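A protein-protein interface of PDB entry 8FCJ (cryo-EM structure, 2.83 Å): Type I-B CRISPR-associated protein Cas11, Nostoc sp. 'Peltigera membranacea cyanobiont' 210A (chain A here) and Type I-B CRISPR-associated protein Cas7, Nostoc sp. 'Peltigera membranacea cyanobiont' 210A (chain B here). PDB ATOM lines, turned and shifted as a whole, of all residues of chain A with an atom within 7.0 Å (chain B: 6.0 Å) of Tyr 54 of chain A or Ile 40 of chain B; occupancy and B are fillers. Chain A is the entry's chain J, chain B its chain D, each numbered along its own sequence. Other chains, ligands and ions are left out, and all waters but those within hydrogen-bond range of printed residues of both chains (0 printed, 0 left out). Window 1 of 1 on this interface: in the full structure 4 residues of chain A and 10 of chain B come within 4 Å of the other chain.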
ATOM      1  N   ARG A  47     -30.467  18.077   3.455  1.00  0.00           N
ATOM      2  CA  ARG A  47     -30.588  18.212   4.901  1.00  0.00           C
ATOM      3  C   ARG A  47     -29.220  18.355   5.554  1.00  0.00           C
ATOM      4  O   ARG A  47     -29.038  19.176   6.461  1.00  0.00           O
ATOM      5  CB  ARG A  47     -31.333  17.004   5.468  1.00  0.00           C
ATOM      6  CG  ARG A  47     -31.365  16.924   6.981  1.00  0.00           C
ATOM      7  CD  ARG A  47     -32.749  16.523   7.466  1.00  0.00           C
ATOM      8  NE  ARG A  47     -33.805  17.231   6.752  1.00  0.00           N
ATOM      9  CZ  ARG A  47     -35.043  17.381   7.201  1.00  0.00           C
ATOM     10  NH1 ARG A  47     -35.427  16.862   8.357  1.00  0.00           N
ATOM     11  NH2 ARG A  47     -35.920  18.064   6.471  1.00  0.00           N
ATOM     12  N   LEU A  48     -28.245  17.562   5.104  1.00  0.00           N
ATOM     13  CA  LEU A  48     -26.896  17.666   5.655  1.00  0.00           C
ATOM     14  C   LEU A  48     -26.295  19.039   5.383  1.00  0.00           C
ATOM     15  O   LEU A  48     -25.676  19.639   6.269  1.00  0.00           O
ATOM     16  CB  LEU A  48     -26.007  16.567   5.076  1.00  0.00           C
ATOM     17  CG  LEU A  48     -24.571  16.507   5.598  1.00  0.00           C
ATOM     18  CD1 LEU A  48     -24.543  16.614   7.112  1.00  0.00           C
ATOM     19  CD2 LEU A  48     -23.891  15.232   5.140  1.00  0.00           C
ATOM     20  N   ARG A  49     -26.473  19.554   4.165  1.00  0.00           N
ATOM     21  CA  ARG A  49     -25.962  20.884   3.848  1.00  0.00           C
ATOM     22  C   ARG A  49     -26.628  21.949   4.705  1.00  0.00           C
ATOM     23  O   ARG A  49     -25.958  22.855   5.219  1.00  0.00           O
ATOM     24  CB  ARG A  49     -26.177  21.195   2.369  1.00  0.00           C
ATOM     25  CG  ARG A  49     -25.545  22.503   1.933  1.00  0.00           C
ATOM     26  CD  ARG A  49     -26.042  22.930   0.568  1.00  0.00           C
ATOM     27  NE  ARG A  49     -27.469  23.225   0.589  1.00  0.00           N
ATOM     28  CZ  ARG A  49     -27.980  24.423   0.836  1.00  0.00           C
ATOM     29  NH1 ARG A  49     -27.206  25.465   1.091  1.00  0.00           N
ATOM     30  NH2 ARG A  49     -29.300  24.579   0.827  1.00  0.00           N
ATOM     31  N   ALA A  50     -27.949  21.860   4.870  1.00  0.00           N
ATOM     32  CA  ALA A  50     -28.660  22.847   5.673  1.00  0.00           C
ATOM     33  C   ALA A  50     -28.193  22.814   7.120  1.00  0.00           C
ATOM     34  O   ALA A  50     -28.015  23.864   7.747  1.00  0.00           O
ATOM     35  CB  ALA A  50     -30.167  22.609   5.586  1.00  0.00           C
ATOM     36  N   GLU A  51     -27.986  21.616   7.670  1.00  0.00           N
ATOM     37  CA  GLU A  51     -27.499  21.515   9.040  1.00  0.00           C
ATOM     38  C   GLU A  51     -26.074  22.041   9.162  1.00  0.00           C
ATOM     39  O   GLU A  51     -25.714  22.634  10.185  1.00  0.00           O
ATOM     40  CB  GLU A  51     -27.583  20.071   9.524  1.00  0.00           C
ATOM     41  CG  GLU A  51     -28.996  19.562   9.725  1.00  0.00           C
ATOM     42  CD  GLU A  51     -29.042  18.069   9.979  1.00  0.00           C
ATOM     43  OE1 GLU A  51     -30.144  17.486   9.913  1.00  0.00           O
ATOM     44  OE2 GLU A  51     -27.973  17.479  10.242  1.00  0.00           O
ATOM     45  N   LEU A  52     -25.246  21.824   8.138  1.00  0.00           N
ATOM     46  CA  LEU A  52     -23.893  22.370   8.162  1.00  0.00           C
ATOM     47  C   LEU A  52     -23.911  23.892   8.138  1.00  0.00           C
ATOM     48  O   LEU A  52     -23.102  24.541   8.812  1.00  0.00           O
ATOM     49  CB  LEU A  52     -23.083  21.825   6.988  1.00  0.00           C
ATOM     50  CG  LEU A  52     -22.329  20.521   7.244  1.00  0.00           C
ATOM     51  CD1 LEU A  52     -21.505  20.137   6.032  1.00  0.00           C
ATOM     52  CD2 LEU A  52     -21.450  20.643   8.474  1.00  0.00           C
ATOM     53  N   ASN A  53     -24.825  24.482   7.366  1.00  0.00           N
ATOM     54  CA  ASN A  53     -24.931  25.935   7.300  1.00  0.00           C
ATOM     55  C   ASN A  53     -25.622  26.535   8.518  1.00  0.00           C
ATOM     56  O   ASN A  53     -25.658  27.763   8.645  1.00  0.00           O
ATOM     57  CB  ASN A  53     -25.676  26.348   6.032  1.00  0.00           C
ATOM     58  CG  ASN A  53     -24.841  26.171   4.782  1.00  0.00           C
ATOM     59  OD1 ASN A  53     -23.647  25.884   4.857  1.00  0.00           O
ATOM     60  ND2 ASN A  53     -25.466  26.339   3.624  1.00  0.00           N
ATOM     61  N   TYR A  54     -26.165  25.707   9.410  1.00  0.00           N
ATOM     62  CA  TYR A  54     -26.935  26.181  10.552  1.00  0.00           C
ATOM     63  C   TYR A  54     -26.070  26.678  11.701  1.00  0.00           C
ATOM     64  O   TYR A  54     -26.615  27.209  12.674  1.00  0.00           O
ATOM     65  CB  TYR A  54     -27.842  25.061  11.062  1.00  0.00           C
ATOM     66  CG  TYR A  54     -29.173  24.985  10.361  1.00  0.00           C
ATOM     67  CD1 TYR A  54     -29.614  26.023   9.559  1.00  0.00           C
ATOM     68  CD2 TYR A  54     -29.977  23.859  10.478  1.00  0.00           C
ATOM     69  CE1 TYR A  54     -30.826  25.955   8.913  1.00  0.00           C
ATOM     70  CE2 TYR A  54     -31.191  23.781   9.829  1.00  0.00           C
ATOM     71  CZ  TYR A  54     -31.610  24.833   9.047  1.00  0.00           C
ATOM     72  OH  TYR A  54     -32.820  24.766   8.397  1.00  0.00           O
ATOM     73  N   CYS A  55     -24.756  26.519  11.620  1.00  0.00           N
ATOM     74  CA  CYS A  55     -23.885  26.754  12.759  1.00  0.00           C
ATOM     75  C   CYS A  55     -23.366  28.188  12.781  1.00  0.00           C
ATOM     76  O   CYS A  55     -23.376  28.899  11.774  1.00  0.00           O
ATOM     77  CB  CYS A  55     -22.724  25.768  12.735  1.00  0.00           C
ATOM     78  SG  CYS A  55     -23.259  24.059  12.490  1.00  0.00           S
ATOM     79  N   TYR A  56     -22.903  28.604  13.957  1.00  0.00           N
ATOM     80  CA  TYR A  56     -22.473  29.973  14.225  1.00  0.00           C
ATOM     81  C   TYR A  56     -21.142  29.984  14.974  1.00  0.00           C
ATOM     82  O   TYR A  56     -20.987  30.624  16.016  1.00  0.00           O
ATOM     83  CB  TYR A  56     -23.564  30.734  14.975  1.00  0.00           C
ATOM     84  CG  TYR A  56     -24.111  30.026  16.196  1.00  0.00           C
ATOM     85  CD1 TYR A  56     -25.168  29.136  16.086  1.00  0.00           C
ATOM     86  CD2 TYR A  56     -23.575  30.252  17.456  1.00  0.00           C
ATOM     87  CE1 TYR A  56     -25.673  28.488  17.194  1.00  0.00           C
ATOM     88  CE2 TYR A  56     -24.075  29.609  18.569  1.00  0.00           C
ATOM     89  CZ  TYR A  56     -25.123  28.728  18.433  1.00  0.00           C
ATOM     90  OH  TYR A  56     -25.621  28.086  19.541  1.00  0.00           O
ATOM     91  N   ASP A  57     -20.179  29.214  14.458  1.00  0.00           N
ATOM     92  CA  ASP A  57     -18.759  29.301  14.801  1.00  0.00           C
ATOM     93  C   ASP A  57     -18.380  28.542  16.066  1.00  0.00           C
ATOM     94  O   ASP A  57     -19.161  28.465  17.021  1.00  0.00           O
ATOM     95  CB  ASP A  57     -18.313  30.765  14.929  1.00  0.00           C
ATOM     96  CG  ASP A  57     -16.955  30.910  15.602  1.00  0.00           C
ATOM     97  OD1 ASP A  57     -16.033  30.131  15.281  1.00  0.00           O
ATOM     98  OD2 ASP A  57     -16.811  31.804  16.464  1.00  0.00           O
ATOM     99  N   SER A  60     -20.584  25.551  18.006  1.00  0.00           N
ATOM    100  CA  SER A  60     -21.393  25.073  16.898  1.00  0.00           C
ATOM    101  C   SER A  60     -20.497  24.701  15.726  1.00  0.00           C
ATOM    102  O   SER A  60     -19.489  25.357  15.454  1.00  0.00           O
ATOM    103  CB  SER A  60     -22.404  26.136  16.474  1.00  0.00           C
ATOM    104  OG  SER A  60     -21.748  27.235  15.875  1.00  0.00           O
ATOM    105  N   PHE A  61     -20.885  23.629  15.047  1.00  0.00           N
ATOM    106  CA  PHE A  61     -20.192  22.978  13.941  1.00  0.00           C
ATOM    107  C   PHE A  61     -18.977  22.182  14.397  1.00  0.00           C
ATOM    108  O   PHE A  61     -18.684  21.155  13.788  1.00  0.00           O
ATOM    109  CB  PHE A  61     -19.766  23.999  12.880  1.00  0.00           C
ATOM    110  CG  PHE A  61     -18.851  23.439  11.839  1.00  0.00           C
ATOM    111  CD1 PHE A  61     -19.360  22.713  10.781  1.00  0.00           C
ATOM    112  CD2 PHE A  61     -17.487  23.640  11.914  1.00  0.00           C
ATOM    113  CE1 PHE A  61     -18.528  22.190   9.824  1.00  0.00           C
ATOM    114  CE2 PHE A  61     -16.650  23.119  10.957  1.00  0.00           C
ATOM    115  CZ  PHE A  61     -17.173  22.395   9.910  1.00  0.00           C
ATOM    116  N   ARG A  98     -15.655  23.635   7.258  1.00  0.00           N
ATOM    117  CA  ARG A  98     -16.957  23.584   6.598  1.00  0.00           C
ATOM    118  C   ARG A  98     -16.806  23.524   5.083  1.00  0.00           C
ATOM    119  O   ARG A  98     -17.555  22.811   4.405  1.00  0.00           O
ATOM    120  CB  ARG A  98     -17.803  24.789   7.003  1.00  0.00           C
ATOM    121  CG  ARG A  98     -19.231  24.725   6.494  1.00  0.00           C
ATOM    122  CD  ARG A  98     -20.168  25.551   7.353  1.00  0.00           C
ATOM    123  NE  ARG A  98     -19.906  26.979   7.230  1.00  0.00           N
ATOM    124  CZ  ARG A  98     -20.568  27.920   7.890  1.00  0.00           C
ATOM    125  NH1 ARG A  98     -21.540  27.617   8.734  1.00  0.00           N
ATOM    126  NH2 ARG A  98     -20.247  29.195   7.698  1.00  0.00           N
ATOM    127  N   ASN B  30     -36.776  38.437  15.054  1.00  0.00           N
ATOM    128  CA  ASN B  30     -36.258  38.552  13.699  1.00  0.00           C
ATOM    129  C   ASN B  30     -35.502  37.284  13.338  1.00  0.00           C
ATOM    130  O   ASN B  30     -34.632  36.840  14.093  1.00  0.00           O
ATOM    131  CB  ASN B  30     -35.348  39.771  13.559  1.00  0.00           C
ATOM    132  CG  ASN B  30     -36.056  40.953  12.941  1.00  0.00           C
ATOM    133  OD1 ASN B  30     -35.434  41.798  12.301  1.00  0.00           O
ATOM    134  ND2 ASN B  30     -37.364  41.028  13.139  1.00  0.00           N
ATOM    135  N   HIS B  31     -35.835  36.710  12.190  1.00  0.00           N
ATOM    136  CA  HIS B  31     -35.214  35.489  11.712  1.00  0.00           C
ATOM    137  C   HIS B  31     -34.394  35.767  10.460  1.00  0.00           C
ATOM    138  O   HIS B  31     -34.616  36.745   9.744  1.00  0.00           O
ATOM    139  CB  HIS B  31     -36.264  34.415  11.415  1.00  0.00           C
ATOM    140  CG  HIS B  31     -37.121  34.067  12.590  1.00  0.00           C
ATOM    141  ND1 HIS B  31     -38.459  34.385  12.654  1.00  0.00           N
ATOM    142  CD2 HIS B  31     -36.830  33.430  13.748  1.00  0.00           C
ATOM    143  CE1 HIS B  31     -38.957  33.957  13.801  1.00  0.00           C
ATOM    144  NE2 HIS B  31     -37.988  33.374  14.482  1.00  0.00           N
ATOM    145  N   ASP B  32     -33.433  34.885  10.210  1.00  0.00           N
ATOM    146  CA  ASP B  32     -32.610  34.956   9.012  1.00  0.00           C
ATOM    147  C   ASP B  32     -33.373  34.313   7.854  1.00  0.00           C
ATOM    148  O   ASP B  32     -34.583  34.088   7.929  1.00  0.00           O
ATOM    149  CB  ASP B  32     -31.259  34.296   9.261  1.00  0.00           C
ATOM    150  CG  ASP B  32     -30.157  34.889   8.412  1.00  0.00           C
ATOM    151  OD1 ASP B  32     -30.392  35.117   7.208  1.00  0.00           O
ATOM    152  OD2 ASP B  32     -29.056  35.131   8.948  1.00  0.00           O
ATOM    153  N   ILE B  33     -32.670  34.032   6.754  1.00  0.00           N
ATOM    154  CA  ILE B  33     -33.300  33.386   5.609  1.00  0.00           C
ATOM    155  C   ILE B  33     -33.905  32.060   6.047  1.00  0.00           C
ATOM    156  O   ILE B  33     -33.241  31.232   6.682  1.00  0.00           O
ATOM    157  CB  ILE B  33     -32.280  33.196   4.478  1.00  0.00           C
ATOM    158  CG1 ILE B  33     -31.905  34.548   3.873  1.00  0.00           C
ATOM    159  CG2 ILE B  33     -32.841  32.285   3.405  1.00  0.00           C
ATOM    160  CD1 ILE B  33     -33.050  35.235   3.173  1.00  0.00           C
ATOM    161  N   ARG B  34     -35.176  31.855   5.708  1.00  0.00           N
ATOM    162  CA  ARG B  34     -35.947  30.715   6.190  1.00  0.00           C
ATOM    163  C   ARG B  34     -35.964  29.621   5.130  1.00  0.00           C
ATOM    164  O   ARG B  34     -36.609  29.767   4.087  1.00  0.00           O
ATOM    165  CB  ARG B  34     -37.371  31.137   6.547  1.00  0.00           C
ATOM    166  CG  ARG B  34     -37.464  32.135   7.683  1.00  0.00           C
ATOM    167  CD  ARG B  34     -38.815  32.042   8.369  1.00  0.00           C
ATOM    168  NE  ARG B  34     -39.780  32.975   7.800  1.00  0.00           N
ATOM    169  CZ  ARG B  34     -40.148  34.112   8.371  1.00  0.00           C
ATOM    170  NH1 ARG B  34     -39.658  34.488   9.541  1.00  0.00           N
ATOM    171  NH2 ARG B  34     -41.030  34.892   7.754  1.00  0.00           N
ATOM    172  N   ARG B  35     -35.259  28.527   5.404  1.00  0.00           N
ATOM    173  CA  ARG B  35     -35.340  27.320   4.592  1.00  0.00           C
ATOM    174  C   ARG B  35     -34.739  26.168   5.384  1.00  0.00           C
ATOM    175  O   ARG B  35     -33.735  26.342   6.076  1.00  0.00           O
ATOM    176  CB  ARG B  35     -34.640  27.463   3.227  1.00  0.00           C
ATOM    177  CG  ARG B  35     -33.108  27.594   3.209  1.00  0.00           C
ATOM    178  CD  ARG B  35     -32.569  28.737   4.055  1.00  0.00           C
ATOM    179  NE  ARG B  35     -31.201  28.503   4.499  1.00  0.00           N
ATOM    180  CZ  ARG B  35     -30.882  27.867   5.617  1.00  0.00           C
ATOM    181  NH1 ARG B  35     -31.810  27.403   6.434  1.00  0.00           N
ATOM    182  NH2 ARG B  35     -29.598  27.699   5.924  1.00  0.00           N
ATOM    183  N   GLY B  36     -35.369  25.001   5.286  1.00  0.00           N
ATOM    184  CA  GLY B  36     -34.919  23.838   6.023  1.00  0.00           C
ATOM    185  C   GLY B  36     -35.743  23.568   7.265  1.00  0.00           C
ATOM    186  O   GLY B  36     -36.946  23.840   7.290  1.00  0.00           O
ATOM    187  N   ASN B  37     -35.106  23.031   8.304  1.00  0.00           N
ATOM    188  CA  ASN B  37     -35.796  22.728   9.551  1.00  0.00           C
ATOM    189  C   ASN B  37     -35.745  23.895  10.530  1.00  0.00           C
ATOM    190  O   ASN B  37     -36.768  24.271  11.107  1.00  0.00           O
ATOM    191  CB  ASN B  37     -35.188  21.485  10.202  1.00  0.00           C
ATOM    192  CG  ASN B  37     -35.156  20.298   9.271  1.00  0.00           C
ATOM    193  OD1 ASN B  37     -35.871  20.260   8.270  1.00  0.00           O
ATOM    194  ND2 ASN B  37     -34.318  19.321   9.590  1.00  0.00           N
ATOM    195  N   LYS B  38     -34.565  24.469  10.732  1.00  0.00           N
ATOM    196  CA  LYS B  38     -34.397  25.528  11.714  1.00  0.00           C
ATOM    197  C   LYS B  38     -34.832  26.870  11.148  1.00  0.00           C
ATOM    198  O   LYS B  38     -34.605  27.170   9.973  1.00  0.00           O
ATOM    199  CB  LYS B  38     -32.940  25.613  12.162  1.00  0.00           C
ATOM    200  CG  LYS B  38     -32.568  24.688  13.300  1.00  0.00           C
ATOM    201  CD  LYS B  38     -31.560  25.349  14.218  1.00  0.00           C
ATOM    202  CE  LYS B  38     -30.567  24.342  14.764  1.00  0.00           C
ATOM    203  NZ  LYS B  38     -29.213  24.941  14.919  1.00  0.00           N
ATOM    204  N   THR B  39     -35.468  27.676  11.993  1.00  0.00           N
ATOM    205  CA  THR B  39     -35.659  29.095  11.712  1.00  0.00           C
ATOM    206  C   THR B  39     -34.542  29.831  12.439  1.00  0.00           C
ATOM    207  O   THR B  39     -34.582  29.996  13.660  1.00  0.00           O
ATOM    208  CB  THR B  39     -37.035  29.571  12.159  1.00  0.00           C
ATOM    209  OG1 THR B  39     -37.251  29.192  13.523  1.00  0.00           O
ATOM    210  CG2 THR B  39     -38.116  28.952  11.291  1.00  0.00           C
ATOM    211  N   ILE B  40     -33.536  30.267  11.686  1.00  0.00           N
ATOM    212  CA  ILE B  40     -32.326  30.807  12.288  1.00  0.00           C
ATOM    213  C   ILE B  40     -32.595  32.207  12.817  1.00  0.00           C
ATOM    214  O   ILE B  40     -33.086  33.081  12.092  1.00  0.00           O
ATOM    215  CB  ILE B  40     -31.178  30.806  11.268  1.00  0.00           C
ATOM    216  CG1 ILE B  40     -30.677  29.381  11.038  1.00  0.00           C
ATOM    217  CG2 ILE B  40     -30.041  31.692  11.738  1.00  0.00           C
ATOM    218  CD1 ILE B  40     -30.544  28.572  12.305  1.00  0.00           C
ATOM    219  N   LEU B  41     -32.281  32.423  14.090  1.00  0.00           N
ATOM    220  CA  LEU B  41     -32.371  33.753  14.670  1.00  0.00           C
ATOM    221  C   LEU B  41     -31.334  34.671  14.038  1.00  0.00           C
ATOM    222  O   LEU B  41     -30.203  34.259  13.765  1.00  0.00           O
ATOM    223  CB  LEU B  41     -32.158  33.683  16.179  1.00  0.00           C
ATOM    224  CG  LEU B  41     -33.126  34.461  17.065  1.00  0.00           C
ATOM    225  CD1 LEU B  41     -34.551  34.057  16.760  1.00  0.00           C
ATOM    226  CD2 LEU B  41     -32.802  34.211  18.523  1.00  0.00           C
ATOM    227  N   GLN B  42     -31.721  35.919  13.798  1.00  0.00           N
ATOM    228  CA  GLN B  42     -30.793  36.902  13.252  1.00  0.00           C
ATOM    229  C   GLN B  42     -29.742  37.219  14.306  1.00  0.00           C
ATOM    230  O   GLN B  42     -30.022  37.920  15.281  1.00  0.00           O
ATOM    231  CB  GLN B  42     -31.545  38.158  12.827  1.00  0.00           C
ATOM    232  CG  GLN B  42     -30.657  39.349  12.517  1.00  0.00           C
ATOM    233  CD  GLN B  42     -29.887  39.181  11.227  1.00  0.00           C
ATOM    234  OE1 GLN B  42     -30.470  39.157  10.143  1.00  0.00           O
ATOM    235  NE2 GLN B  42     -28.572  39.066  11.333  1.00  0.00           N
ATOM    236  N   LYS B  43     -28.533  36.695  14.122  1.00  0.00           N
ATOM    237  CA  LYS B  43     -27.490  36.825  15.125  1.00  0.00           C
ATOM    238  C   LYS B  43     -26.159  37.125  14.455  1.00  0.00           C
ATOM    239  O   LYS B  43     -25.959  36.865  13.267  1.00  0.00           O
ATOM    240  CB  LYS B  43     -27.369  35.561  15.983  1.00  0.00           C
ATOM    241  CG  LYS B  43     -27.292  34.275  15.190  1.00  0.00           C
ATOM    242  CD  LYS B  43     -27.351  33.070  16.105  1.00  0.00           C
ATOM    243  CE  LYS B  43     -27.565  31.792  15.319  1.00  0.00           C
ATOM    244  NZ  LYS B  43     -28.994  31.588  14.975  1.00  0.00           N
ATOM    245  N   GLU B 174     -35.561  28.688  16.773  1.00  0.00           N
ATOM    246  CA  GLU B 174     -34.580  29.267  17.678  1.00  0.00           C
ATOM    247  C   GLU B 174     -35.218  30.386  18.487  1.00  0.00           C
ATOM    248  O   GLU B 174     -35.912  31.243  17.934  1.00  0.00           O
ATOM    249  CB  GLU B 174     -33.380  29.802  16.898  1.00  0.00           C
ATOM    250  CG  GLU B 174     -32.360  28.746  16.531  1.00  0.00           C
ATOM    251  CD  GLU B 174     -31.126  29.334  15.881  1.00  0.00           C
ATOM    252  OE1 GLU B 174     -31.081  30.568  15.697  1.00  0.00           O
ATOM    253  OE2 GLU B 174     -30.198  28.563  15.561  1.00  0.00           O
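The side-chain amide oxygen of Asn 37 of chain B sits at hydrogen-bond distance from the guanidinium group of Arg 47 of chain A, 2.8 Å away. N of Lys 38 of chain B is in hydrogen-bond range of OH of Tyr 54 of chain A (2.9 Å). OH of Tyr 54 of chain A is in hydrogen-bond range of N of Asn 37 of chain B (2.9 Å). The backbone carbonyl oxygen of Arg 35 of chain B is in hydrogen-bond range of the side-chain hydroxyl of Tyr 54 of chain A, 3.0 Å away.
N of Asp 32 of chain B lies within hydrogen-bond range of O of Ile 40 of chain B, at 2.6 Å. NZ of Lys 43 of chain B lies within salt-bridge range of OE1 of Glu 174 of chain B. The backbone carbonyl oxygen of Leu 41 of chain B sits at hydrogen-bond distance from the side-chain amino group of Lys 43 of chain B (3.2 Å). The backbone NH of Tyr 56 of chain A sits at hydrogen-bond distance from the side-chain hydroxyl of Ser 60 of chain A (2.6 Å). The side-chain carboxylate of Glu 174 of chain B lies within salt-bridge range of the side-chain amino group of Lys 38 of chain B (3.8 Å).
Tyr 54 of chain A touches Gly 36 of chain B. Tyr 54 of chain A touches Ile 40 of chain B. Lys 43 of chain B touches Tyr 56 of chain A (CE to CD1, 3.7 Å).
Printed residues of chain B within 4 Å of Arg 47 of chain A: Asn 37. Of chain B, only Arg 35, Gly 36, Asn 37, Lys 38 and Ile 40 come within 4 Å of Tyr 54 of chain A. Printed residues of chain B within 4 Å of Tyr 56 of chain A: Lys 43. Asp 57 of chain A touches none of the printed residues of chain B. Of the printed residues of chain A, Gly 36 of chain B touches Tyr 54 (3.3 Å). Ile 40 of chain B touches one residue of chain A. Of the printed residues of chain A, Lys 43 of chain B touches Tyr 56. Glu 174 of chain B touches none of the printed residues of chain A. The nearest residue of chain B that does not touch Tyr 54 of chain A is Glu 174 of chain B (4.8 Å). The nearest printed residue of chain A that does not touch Gly 36 of chain B is Ala 50 of chain A (4.9 Å).
Printed residues of chain A that touch a printed residue of chain B: Arg 47, Tyr 54 and Tyr 56. Hydrophobic or aromatic side chains of chain A that line the printed part of chain B: Tyr 54 and Tyr 56. Hydrophobic or aromatic side chains of chain B within 4 Å of the printed part of chain A: Ile 40. Among the printed residues, no Asp or Glu carboxylate lies within 4 Å of a Lys or Arg side-chain nitrogen of the other chain.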
